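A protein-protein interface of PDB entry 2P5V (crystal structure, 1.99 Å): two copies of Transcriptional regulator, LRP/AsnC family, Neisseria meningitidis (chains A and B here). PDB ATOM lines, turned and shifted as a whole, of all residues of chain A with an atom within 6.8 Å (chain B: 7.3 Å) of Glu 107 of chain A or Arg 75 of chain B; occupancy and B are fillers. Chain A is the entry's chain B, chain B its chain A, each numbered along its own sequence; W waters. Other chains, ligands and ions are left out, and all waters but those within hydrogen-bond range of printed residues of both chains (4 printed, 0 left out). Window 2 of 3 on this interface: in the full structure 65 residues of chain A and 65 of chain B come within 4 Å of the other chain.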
ATOM      1  N   ARG A  75     -17.421 -15.891   9.931  1.00  0.00           N
ATOM      2  CA  ARG A  75     -16.111 -15.732   9.337  1.00  0.00           C
ATOM      3  C   ARG A  75     -15.710 -14.280   9.447  1.00  0.00           C
ATOM      4  O   ARG A  75     -16.291 -13.416   8.800  1.00  0.00           O
ATOM      5  CB  ARG A  75     -16.155 -16.137   7.881  1.00  0.00           C
ATOM      6  CG  ARG A  75     -16.532 -17.593   7.655  1.00  0.00           C
ATOM      7  CD  ARG A  75     -16.522 -17.882   6.159  1.00  0.00           C
ATOM      8  NE  ARG A  75     -17.228 -19.091   5.770  1.00  0.00           N
ATOM      9  CZ  ARG A  75     -17.252 -19.583   4.528  1.00  0.00           C
ATOM     10  NH1 ARG A  75     -16.600 -18.978   3.542  1.00  0.00           N
ATOM     11  NH2 ARG A  75     -17.929 -20.696   4.263  1.00  0.00           N
ATOM     12  N   VAL A  76     -14.710 -14.025  10.272  1.00  0.00           N
ATOM     13  CA  VAL A  76     -14.313 -12.667  10.598  1.00  0.00           C
ATOM     14  C   VAL A  76     -13.001 -12.328   9.911  1.00  0.00           C
ATOM     15  O   VAL A  76     -12.047 -13.102   9.953  1.00  0.00           O
ATOM     16  CB  VAL A  76     -14.172 -12.486  12.122  1.00  0.00           C
ATOM     17  CG1 VAL A  76     -13.468 -11.187  12.437  1.00  0.00           C
ATOM     18  CG2 VAL A  76     -15.549 -12.554  12.784  1.00  0.00           C
ATOM     19  N   SER A  77     -12.972 -11.158   9.280  1.00  0.00           N
ATOM     20  CA  SER A  77     -11.779 -10.648   8.644  1.00  0.00           C
ATOM     21  C   SER A  77     -11.222  -9.547   9.559  1.00  0.00           C
ATOM     22  O   SER A  77     -11.919  -8.575   9.879  1.00  0.00           O
ATOM     23  CB  SER A  77     -12.131 -10.160   7.228  1.00  0.00           C
ATOM     24  OG  SER A  77     -11.010  -9.631   6.560  1.00  0.00           O
ATOM     25  N   LEU A 104      -7.680 -19.433  11.419  1.00  0.00           N
ATOM     26  CA  LEU A 104      -7.584 -20.510  10.409  1.00  0.00           C
ATOM     27  C   LEU A 104      -6.597 -20.166   9.298  1.00  0.00           C
ATOM     28  O   LEU A 104      -6.231 -19.001   9.118  1.00  0.00           O
ATOM     29  CB  LEU A 104      -8.965 -20.827   9.780  1.00  0.00           C
ATOM     30  CG  LEU A 104     -10.074 -21.360  10.695  1.00  0.00           C
ATOM     31  CD1 LEU A 104     -11.310 -21.703   9.909  1.00  0.00           C
ATOM     32  CD2 LEU A 104      -9.624 -22.564  11.491  1.00  0.00           C
ATOM     33  N   THR A 105      -6.216 -21.198   8.541  1.00  0.00           N
ATOM     34  CA  THR A 105      -5.186 -21.125   7.507  1.00  0.00           C
ATOM     35  C   THR A 105      -5.626 -20.590   6.146  1.00  0.00           C
ATOM     36  O   THR A 105      -4.773 -20.259   5.322  1.00  0.00           O
ATOM     37  CB  THR A 105      -4.617 -22.543   7.215  1.00  0.00           C
ATOM     38  OG1 THR A 105      -5.700 -23.426   6.921  1.00  0.00           O
ATOM     39  CG2 THR A 105      -3.857 -23.078   8.396  1.00  0.00           C
ATOM     40  N   GLY A 106      -6.933 -20.554   5.884  1.00  0.00           N
ATOM     41  CA  GLY A 106      -7.450 -20.156   4.568  1.00  0.00           C
ATOM     42  C   GLY A 106      -7.760 -18.672   4.456  1.00  0.00           C
ATOM     43  O   GLY A 106      -7.082 -17.842   5.066  1.00  0.00           O
ATOM     44  N   GLU A 107      -8.795 -18.339   3.680  1.00  0.00           N
ATOM     45  CA  GLU A 107      -9.176 -16.939   3.462  1.00  0.00           C
ATOM     46  C   GLU A 107      -9.812 -16.306   4.703  1.00  0.00           C
ATOM     47  O   GLU A 107      -9.722 -15.101   4.900  1.00  0.00           O
ATOM     48  CB  GLU A 107     -10.106 -16.795   2.242  1.00  0.00           C
ATOM     49  CG  GLU A 107     -11.533 -17.383   2.405  1.00  0.00           C
ATOM     50  CD  GLU A 107     -12.321 -17.473   1.069  1.00  0.00           C
ATOM     51  OE1 GLU A 107     -12.052 -16.671   0.140  1.00  0.00           O
ATOM     52  OE2 GLU A 107     -13.213 -18.352   0.953  1.00  0.00           O
ATOM     53  N   THR A 108     -10.449 -17.115   5.542  1.00  0.00           N
ATOM     54  CA  THR A 108     -11.033 -16.608   6.775  1.00  0.00           C
ATOM     55  C   THR A 108      -9.975 -16.490   7.866  1.00  0.00           C
ATOM     56  O   THR A 108      -9.341 -17.481   8.215  1.00  0.00           O
ATOM     57  CB  THR A 108     -12.157 -17.534   7.267  1.00  0.00           C
ATOM     58  OG1 THR A 108     -13.180 -17.585   6.272  1.00  0.00           O
ATOM     59  CG2 THR A 108     -12.737 -17.033   8.588  1.00  0.00           C
ATOM     60  N   ASP A 109      -9.813 -15.288   8.421  1.00  0.00           N
ATOM     61  CA  ASP A 109      -8.856 -15.069   9.510  1.00  0.00           C
ATOM     62  C   ASP A 109      -9.301 -15.757  10.806  1.00  0.00           C
ATOM     63  O   ASP A 109      -8.506 -16.433  11.451  1.00  0.00           O
ATOM     64  CB  ASP A 109      -8.646 -13.575   9.759  1.00  0.00           C
ATOM     65  CG  ASP A 109      -8.242 -12.817   8.493  1.00  0.00           C
ATOM     66  OD1 ASP A 109      -7.899 -13.463   7.470  1.00  0.00           O
ATOM     67  OD2 ASP A 109      -8.276 -11.570   8.527  1.00  0.00           O
ATOM     68  N   TYR A 110     -10.565 -15.574  11.182  1.00  0.00           N
ATOM     69  CA  TYR A 110     -11.132 -16.252  12.353  1.00  0.00           C
ATOM     70  C   TYR A 110     -12.492 -16.835  12.075  1.00  0.00           C
ATOM     71  O   TYR A 110     -13.350 -16.164  11.503  1.00  0.00           O
ATOM     72  CB  TYR A 110     -11.281 -15.286  13.523  1.00  0.00           C
ATOM     73  CG  TYR A 110      -9.985 -14.763  14.053  1.00  0.00           C
ATOM     74  CD1 TYR A 110      -9.311 -15.414  15.085  1.00  0.00           C
ATOM     75  CD2 TYR A 110      -9.432 -13.595  13.537  1.00  0.00           C
ATOM     76  CE1 TYR A 110      -8.105 -14.905  15.594  1.00  0.00           C
ATOM     77  CE2 TYR A 110      -8.242 -13.085  14.025  1.00  0.00           C
ATOM     78  CZ  TYR A 110      -7.578 -13.740  15.051  1.00  0.00           C
ATOM     79  OH  TYR A 110      -6.395 -13.203  15.524  1.00  0.00           O
ATOM     80  N   LEU A 111     -12.693 -18.076  12.519  1.00  0.00           N
ATOM     81  CA  LEU A 111     -14.001 -18.708  12.497  1.00  0.00           C
ATOM     82  C   LEU A 111     -14.583 -18.712  13.904  1.00  0.00           C
ATOM     83  O   LEU A 111     -13.964 -19.234  14.843  1.00  0.00           O
ATOM     84  CB  LEU A 111     -13.913 -20.127  11.937  1.00  0.00           C
ATOM     85  CG  LEU A 111     -15.253 -20.859  11.787  1.00  0.00           C
ATOM     86  CD1 LEU A 111     -16.154 -20.140  10.770  1.00  0.00           C
ATOM     87  CD2 LEU A 111     -15.027 -22.341  11.415  1.00  0.00           C
ATOM     88  N   ALA B  72      -9.118 -29.696  11.695  1.00  0.00           N
ATOM     89  CA  ALA B  72      -9.545 -29.346  10.357  1.00  0.00           C
ATOM     90  C   ALA B  72     -11.012 -28.927  10.332  1.00  0.00           C
ATOM     91  O   ALA B  72     -11.872 -29.521  11.007  1.00  0.00           O
ATOM     92  CB  ALA B  72      -9.341 -30.540   9.425  1.00  0.00           C
ATOM     93  N   PHE B  73     -11.277 -27.903   9.528  1.00  0.00           N
ATOM     94  CA  PHE B  73     -12.624 -27.542   9.146  1.00  0.00           C
ATOM     95  C   PHE B  73     -12.751 -27.914   7.681  1.00  0.00           C
ATOM     96  O   PHE B  73     -12.014 -27.412   6.841  1.00  0.00           O
ATOM     97  CB  PHE B  73     -12.862 -26.060   9.409  1.00  0.00           C
ATOM     98  CG  PHE B  73     -13.030 -25.747  10.871  1.00  0.00           C
ATOM     99  CD1 PHE B  73     -14.284 -25.804  11.460  1.00  0.00           C
ATOM    100  CD2 PHE B  73     -11.931 -25.450  11.664  1.00  0.00           C
ATOM    101  CE1 PHE B  73     -14.450 -25.543  12.826  1.00  0.00           C
ATOM    102  CE2 PHE B  73     -12.085 -25.185  13.028  1.00  0.00           C
ATOM    103  CZ  PHE B  73     -13.354 -25.236  13.605  1.00  0.00           C
ATOM    104  N   ILE B  74     -13.657 -28.833   7.387  1.00  0.00           N
ATOM    105  CA  ILE B  74     -13.766 -29.383   6.051  1.00  0.00           C
ATOM    106  C   ILE B  74     -15.082 -28.942   5.475  1.00  0.00           C
ATOM    107  O   ILE B  74     -16.135 -29.276   6.007  1.00  0.00           O
ATOM    108  CB  ILE B  74     -13.664 -30.923   6.040  1.00  0.00           C
ATOM    109  CG1 ILE B  74     -12.436 -31.364   6.866  1.00  0.00           C
ATOM    110  CG2 ILE B  74     -13.619 -31.437   4.585  1.00  0.00           C
ATOM    111  CD1 ILE B  74     -12.265 -32.859   7.052  1.00  0.00           C
ATOM    112  N   ARG B  75     -15.007 -28.161   4.399  1.00  0.00           N
ATOM    113  CA  ARG B  75     -16.183 -27.719   3.663  1.00  0.00           C
ATOM    114  C   ARG B  75     -16.475 -28.716   2.549  1.00  0.00           C
ATOM    115  O   ARG B  75     -15.720 -28.810   1.570  1.00  0.00           O
ATOM    116  CB  ARG B  75     -15.941 -26.344   3.071  1.00  0.00           C
ATOM    117  CG  ARG B  75     -15.549 -25.278   4.079  1.00  0.00           C
ATOM    118  CD  ARG B  75     -15.325 -23.966   3.339  1.00  0.00           C
ATOM    119  NE  ARG B  75     -14.874 -22.873   4.190  1.00  0.00           N
ATOM    120  CZ  ARG B  75     -14.623 -21.637   3.747  1.00  0.00           C
ATOM    121  NH1 ARG B  75     -14.801 -21.315   2.464  1.00  0.00           N
ATOM    122  NH2 ARG B  75     -14.203 -20.706   4.597  1.00  0.00           N
ATOM    123  N   VAL B  76     -17.581 -29.438   2.687  1.00  0.00           N
ATOM    124  CA  VAL B  76     -17.946 -30.502   1.743  1.00  0.00           C
ATOM    125  C   VAL B  76     -19.108 -30.123   0.848  1.00  0.00           C
ATOM    126  O   VAL B  76     -20.133 -29.657   1.329  1.00  0.00           O
ATOM    127  CB  VAL B  76     -18.346 -31.802   2.479  1.00  0.00           C
ATOM    128  CG1 VAL B  76     -18.830 -32.873   1.486  1.00  0.00           C
ATOM    129  CG2 VAL B  76     -17.168 -32.327   3.265  1.00  0.00           C
ATOM    130  N   SER B  77     -18.942 -30.362  -0.453  1.00  0.00           N
ATOM    131  CA  SER B  77     -20.017 -30.249  -1.416  1.00  0.00           C
ATOM    132  C   SER B  77     -20.568 -31.636  -1.727  1.00  0.00           C
ATOM    133  O   SER B  77     -19.840 -32.540  -2.125  1.00  0.00           O
ATOM    134  CB  SER B  77     -19.523 -29.579  -2.698  1.00  0.00           C
ATOM    135  OG  SER B  77     -20.627 -29.231  -3.514  1.00  0.00           O
ATOM    136  N   LEU B 104     -25.228 -26.330   6.333  1.00  0.00           N
ATOM    137  CA  LEU B 104     -25.201 -24.866   6.526  1.00  0.00           C
ATOM    138  C   LEU B 104     -25.904 -24.116   5.402  1.00  0.00           C
ATOM    139  O   LEU B 104     -26.139 -24.680   4.348  1.00  0.00           O
ATOM    140  CB  LEU B 104     -23.749 -24.363   6.589  1.00  0.00           C
ATOM    141  CG  LEU B 104     -22.843 -24.805   7.743  1.00  0.00           C
ATOM    142  CD1 LEU B 104     -21.522 -24.079   7.623  1.00  0.00           C
ATOM    143  CD2 LEU B 104     -23.481 -24.529   9.083  1.00  0.00           C
ATOM    144  N   GLU B 107     -22.611 -21.248   0.849  1.00  0.00           N
ATOM    145  CA  GLU B 107     -22.115 -22.001  -0.307  1.00  0.00           C
ATOM    146  C   GLU B 107     -21.586 -23.374   0.077  1.00  0.00           C
ATOM    147  O   GLU B 107     -21.559 -24.275  -0.750  1.00  0.00           O
ATOM    148  CB  GLU B 107     -21.043 -21.209  -1.069  1.00  0.00           C
ATOM    149  CG  GLU B 107     -19.791 -20.874  -0.265  1.00  0.00           C
ATOM    150  CD  GLU B 107     -18.770 -20.079  -1.069  1.00  0.00           C
ATOM    151  OE1 GLU B 107     -19.094 -19.638  -2.200  1.00  0.00           O
ATOM    152  OE2 GLU B 107     -17.643 -19.887  -0.557  1.00  0.00           O
ATOM    153  N   THR B 108     -21.147 -23.525   1.320  1.00  0.00           N
ATOM    154  CA  THR B 108     -20.694 -24.823   1.815  1.00  0.00           C
ATOM    155  C   THR B 108     -21.904 -25.621   2.263  1.00  0.00           C
ATOM    156  O   THR B 108     -22.647 -25.175   3.145  1.00  0.00           O
ATOM    157  CB  THR B 108     -19.722 -24.644   2.998  1.00  0.00           C
ATOM    158  OG1 THR B 108     -18.599 -23.855   2.567  1.00  0.00           O
ATOM    159  CG2 THR B 108     -19.273 -25.989   3.539  1.00  0.00           C
ATOM    160  N   ASP B 109     -22.091 -26.795   1.663  1.00  0.00           N
ATOM    161  CA  ASP B 109     -23.216 -27.669   1.985  1.00  0.00           C
ATOM    162  C   ASP B 109     -23.110 -28.249   3.392  1.00  0.00           C
ATOM    163  O   ASP B 109     -24.080 -28.228   4.153  1.00  0.00           O
ATOM    164  CB  ASP B 109     -23.299 -28.821   0.985  1.00  0.00           C
ATOM    165  CG  ASP B 109     -23.460 -28.344  -0.452  1.00  0.00           C
ATOM    166  OD1 ASP B 109     -23.733 -27.141  -0.650  1.00  0.00           O
ATOM    167  OD2 ASP B 109     -23.312 -29.175  -1.372  1.00  0.00           O
ATOM    168  N   TYR B 110     -21.949 -28.806   3.706  1.00  0.00           N
ATOM    169  CA  TYR B 110     -21.674 -29.350   5.028  1.00  0.00           C
ATOM    170  C   TYR B 110     -20.324 -28.900   5.522  1.00  0.00           C
ATOM    171  O   TYR B 110     -19.343 -28.951   4.787  1.00  0.00           O
ATOM    172  CB  TYR B 110     -21.652 -30.874   4.999  1.00  0.00           C
ATOM    173  CG  TYR B 110     -22.963 -31.516   4.668  1.00  0.00           C
ATOM    174  CD1 TYR B 110     -23.854 -31.874   5.674  1.00  0.00           C
ATOM    175  CD2 TYR B 110     -23.315 -31.774   3.350  1.00  0.00           C
ATOM    176  CE1 TYR B 110     -25.068 -32.479   5.372  1.00  0.00           C
ATOM    177  CE2 TYR B 110     -24.516 -32.368   3.038  1.00  0.00           C
ATOM    178  CZ  TYR B 110     -25.395 -32.726   4.051  1.00  0.00           C
ATOM    179  OH  TYR B 110     -26.597 -33.333   3.729  1.00  0.00           O
ATOM    180  N   LEU B 111     -20.285 -28.492   6.783  1.00  0.00           N
ATOM    181  CA  LEU B 111     -19.056 -28.161   7.456  1.00  0.00           C
ATOM    182  C   LEU B 111     -18.762 -29.259   8.470  1.00  0.00           C
ATOM    183  O   LEU B 111     -19.606 -29.576   9.310  1.00  0.00           O
ATOM    184  CB  LEU B 111     -19.168 -26.821   8.166  1.00  0.00           C
ATOM    185  CG  LEU B 111     -17.866 -26.282   8.754  1.00  0.00           C
ATOM    186  CD1 LEU B 111     -16.780 -26.137   7.667  1.00  0.00           C
ATOM    187  CD2 LEU B 111     -18.160 -24.958   9.445  1.00  0.00           C
ATOM    188  N   LEU B 112     -17.565 -29.825   8.372  1.00  0.00           N
ATOM    189  CA  LEU B 112     -17.093 -30.879   9.274  1.00  0.00           C
ATOM    190  C   LEU B 112     -15.965 -30.341  10.131  1.00  0.00           C
ATOM    191  O   LEU B 112     -15.126 -29.581   9.649  1.00  0.00           O
ATOM    192  CB  LEU B 112     -16.562 -32.073   8.478  1.00  0.00           C
ATOM    193  CG  LEU B 112     -17.563 -33.015   7.816  1.00  0.00           C
ATOM    194  CD1 LEU B 112     -18.521 -32.260   6.888  1.00  0.00           C
ATOM    195  CD2 LEU B 112     -16.794 -34.082   7.063  1.00  0.00           C
ATOM    196  N   LEU B 130     -13.079 -39.718   2.446  1.00  0.00           N
ATOM    197  CA  LEU B 130     -14.036 -38.631   2.225  1.00  0.00           C
ATOM    198  C   LEU B 130     -14.320 -38.455   0.732  1.00  0.00           C
ATOM    199  O   LEU B 130     -15.446 -38.663   0.295  1.00  0.00           O
ATOM    200  CB  LEU B 130     -13.537 -37.325   2.865  1.00  0.00           C
ATOM    201  CG  LEU B 130     -14.355 -36.043   2.667  1.00  0.00           C
ATOM    202  CD1 LEU B 130     -15.771 -36.168   3.242  1.00  0.00           C
ATOM    203  CD2 LEU B 130     -13.632 -34.874   3.298  1.00  0.00           C
ATOM    204  N   ASP B 138     -17.163 -32.699  -3.737  1.00  0.00           N
ATOM    205  CA  ASP B 138     -15.841 -32.149  -3.467  1.00  0.00           C
ATOM    206  C   ASP B 138     -15.681 -31.748  -2.016  1.00  0.00           C
ATOM    207  O   ASP B 138     -16.656 -31.640  -1.270  1.00  0.00           O
ATOM    208  CB  ASP B 138     -15.562 -30.935  -4.361  1.00  0.00           C
ATOM    209  CG  ASP B 138     -14.066 -30.588  -4.439  1.00  0.00           C
ATOM    210  OD1 ASP B 138     -13.210 -31.463  -4.128  1.00  0.00           O
ATOM    211  OD2 ASP B 138     -13.749 -29.427  -4.795  1.00  0.00           O
ATOM    212  N   ALA B 139     -14.430 -31.540  -1.623  1.00  0.00           N
ATOM    213  CA  ALA B 139     -14.105 -31.040  -0.306  1.00  0.00           C
ATOM    214  C   ALA B 139     -12.962 -30.041  -0.405  1.00  0.00           C
ATOM    215  O   ALA B 139     -12.070 -30.177  -1.248  1.00  0.00           O
ATOM    216  CB  ALA B 139     -13.726 -32.202   0.614  1.00  0.00           C
ATOM    217  N   GLN B 140     -13.004 -29.031   0.454  1.00  0.00           N
ATOM    218  CA  GLN B 140     -11.860 -28.158   0.681  1.00  0.00           C
ATOM    219  C   GLN B 140     -11.764 -27.864   2.158  1.00  0.00           C
ATOM    220  O   GLN B 140     -12.780 -27.811   2.845  1.00  0.00           O
ATOM    221  CB  GLN B 140     -11.949 -26.872  -0.117  1.00  0.00           C
ATOM    222  CG  GLN B 140     -13.221 -26.094   0.047  1.00  0.00           C
ATOM    223  CD  GLN B 140     -13.214 -24.868  -0.829  1.00  0.00           C
ATOM    224  OE1 GLN B 140     -12.708 -23.825  -0.436  1.00  0.00           O
ATOM    225  NE2 GLN B 140     -13.755 -24.994  -2.033  1.00  0.00           N
ATOM    226  N   SER B 141     -10.540 -27.695   2.649  1.00  0.00           N
ATOM    227  CA  SER B 141     -10.310 -27.696   4.090  1.00  0.00           C
ATOM    228  C   SER B 141      -9.426 -26.572   4.547  1.00  0.00           C
ATOM    229  O   SER B 141      -8.585 -26.048   3.808  1.00  0.00           O
ATOM    230  CB  SER B 141      -9.718 -29.037   4.542  1.00  0.00           C
ATOM    231  OG  SER B 141     -10.568 -30.108   4.151  1.00  0.00           O
ATOM    232  N   SER B 142      -9.620 -26.215   5.804  1.00  0.00           N
ATOM    233  CA  SER B 142      -8.828 -25.209   6.453  1.00  0.00           C
ATOM    234  C   SER B 142      -8.442 -25.790   7.799  1.00  0.00           C
ATOM    235  O   SER B 142      -9.070 -26.747   8.278  1.00  0.00           O
ATOM    236  CB  SER B 142      -9.643 -23.917   6.593  1.00  0.00           C
ATOM    237  OG  SER B 142      -8.811 -22.843   6.981  1.00  0.00           O
HETATM  238  O   HOH W   1      -6.237 -23.640   4.303  1.00  0.00           O
HETATM  239  O   HOH W   2     -17.864 -23.142   5.624  1.00  0.00           O
HETATM  240  O   HOH W   3      -9.502 -19.528   6.829  1.00  0.00           O
HETATM  241  O   HOH W   4     -14.541 -20.401   7.381  1.00  0.00           O
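NH1 of Arg 75 of chain B is in salt-bridge range of OE2 of Glu 107 of chain A.
The side-chain hydroxyl (OG) of Ser 142 of chain B sits at hydrogen-bond distance from the side-chain hydroxyl (OG1) of Thr 105 of chain A (3.2 Å).
OG of Ser 142 of chain B lies within hydrogen-bond range of N of Gly 106 of chain A (3.2 Å).
NH1 of Arg 75 of chain A sits close to NH2 of Arg 75 of chain B (3.1 Å).
The backbone NH of Phe 73 of chain B sits at hydrogen-bond distance from the backbone carbonyl oxygen of Ser 142 of chain B, 2.8 Å away.
The backbone NH (N) of Arg 75 of chain B is in hydrogen-bond range of the backbone carbonyl oxygen (O) of Gln 140 of chain B.
The backbone NH (N) of Leu 104 of chain A is in hydrogen-bond range of the backbone carbonyl oxygen (O) of Asp 109 of chain A, at 3.1 Å.
Among the printed residues, pairs that only touch across the chains: Arg 75 of chain A with Thr 108 of chain B (3.6 Å), Leu 104 of chain A with Phe 73 of chain B (3.7 Å), Leu 104 of chain A with Ser 142 of chain B (3.5 Å), Thr 108 of chain A with Arg 75 of chain B (3.7 Å) and Leu 111 of chain A with Phe 73 of chain B (3.5 Å).
Glu 107 of chain A touches just one residue of chain B: Arg 75.
Arg 75 of chain B touches just these residues of chain A: Arg 75 (3.1 Å), Glu 107 (3.7 Å) and Thr 108 (3.7 Å).
Printed residues of chain B within 4 Å of Leu 104 of chain A: Phe 73 and Ser 142.
Of the printed residues of chain B, Thr 108 of chain A touches Arg 75.
Asp 109 of chain B touches none of the printed residues of chain A.
Of the 19 printed residues of chain B, 4 touch a printed residue of chain A.
Hydrophobic or aromatic side chains of chain B within 4 Å of the printed part of chain A: Phe 73.
Of the 11 printed residues of chain A, 7 touch a printed residue of chain B.
Arg 75 of chain A touches its own counterpart, Arg 75 of chain B.
Arg 75 of chain A touches Thr 108 of chain B, and with the chains exchanged Thr 108 of chain A touches Arg 75 of chain B.
Glu 107 of chain A touches Arg 75 of chain B, but with the chains exchanged Arg 75 of chain A does not touch Glu 107 of chain B (4.3 Å).
Of the 9 pairs that touch across the chains among the printed residues, 3 have their exchanged pair printed and touching as well.
Water W3 lies within hydrogen-bond range of the backbone carbonyl oxygen of Thr 108 of chain A (2.5 Å), the backbone NH of Gly 106 of chain A (2.9 Å), the side-chain hydroxyl of Ser 142 of chain B (3.4 Å) and the backbone NH of Glu 107 of chain A (3.4 Å).
Water W1 bridges the side-chain hydroxyl of Thr 105 of chain A (2.7 Å) and the backbone carbonyl oxygen of Ser 141 of chain B (3.4 Å).
Water W2 lies within hydrogen-bond range of NH2 of Arg 75 of chain A (2.8 Å), OG1 of Thr 108 of chain B (3.2 Å) and NE of Arg 75 of chain B (3.3 Å).
Water W4 lies within hydrogen-bond range of NH2 of Arg 75 of chain B (2.8 Å), OG1 of Thr 108 of chain A (3.3 Å) and NE of Arg 75 of chain A (3.4 Å).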
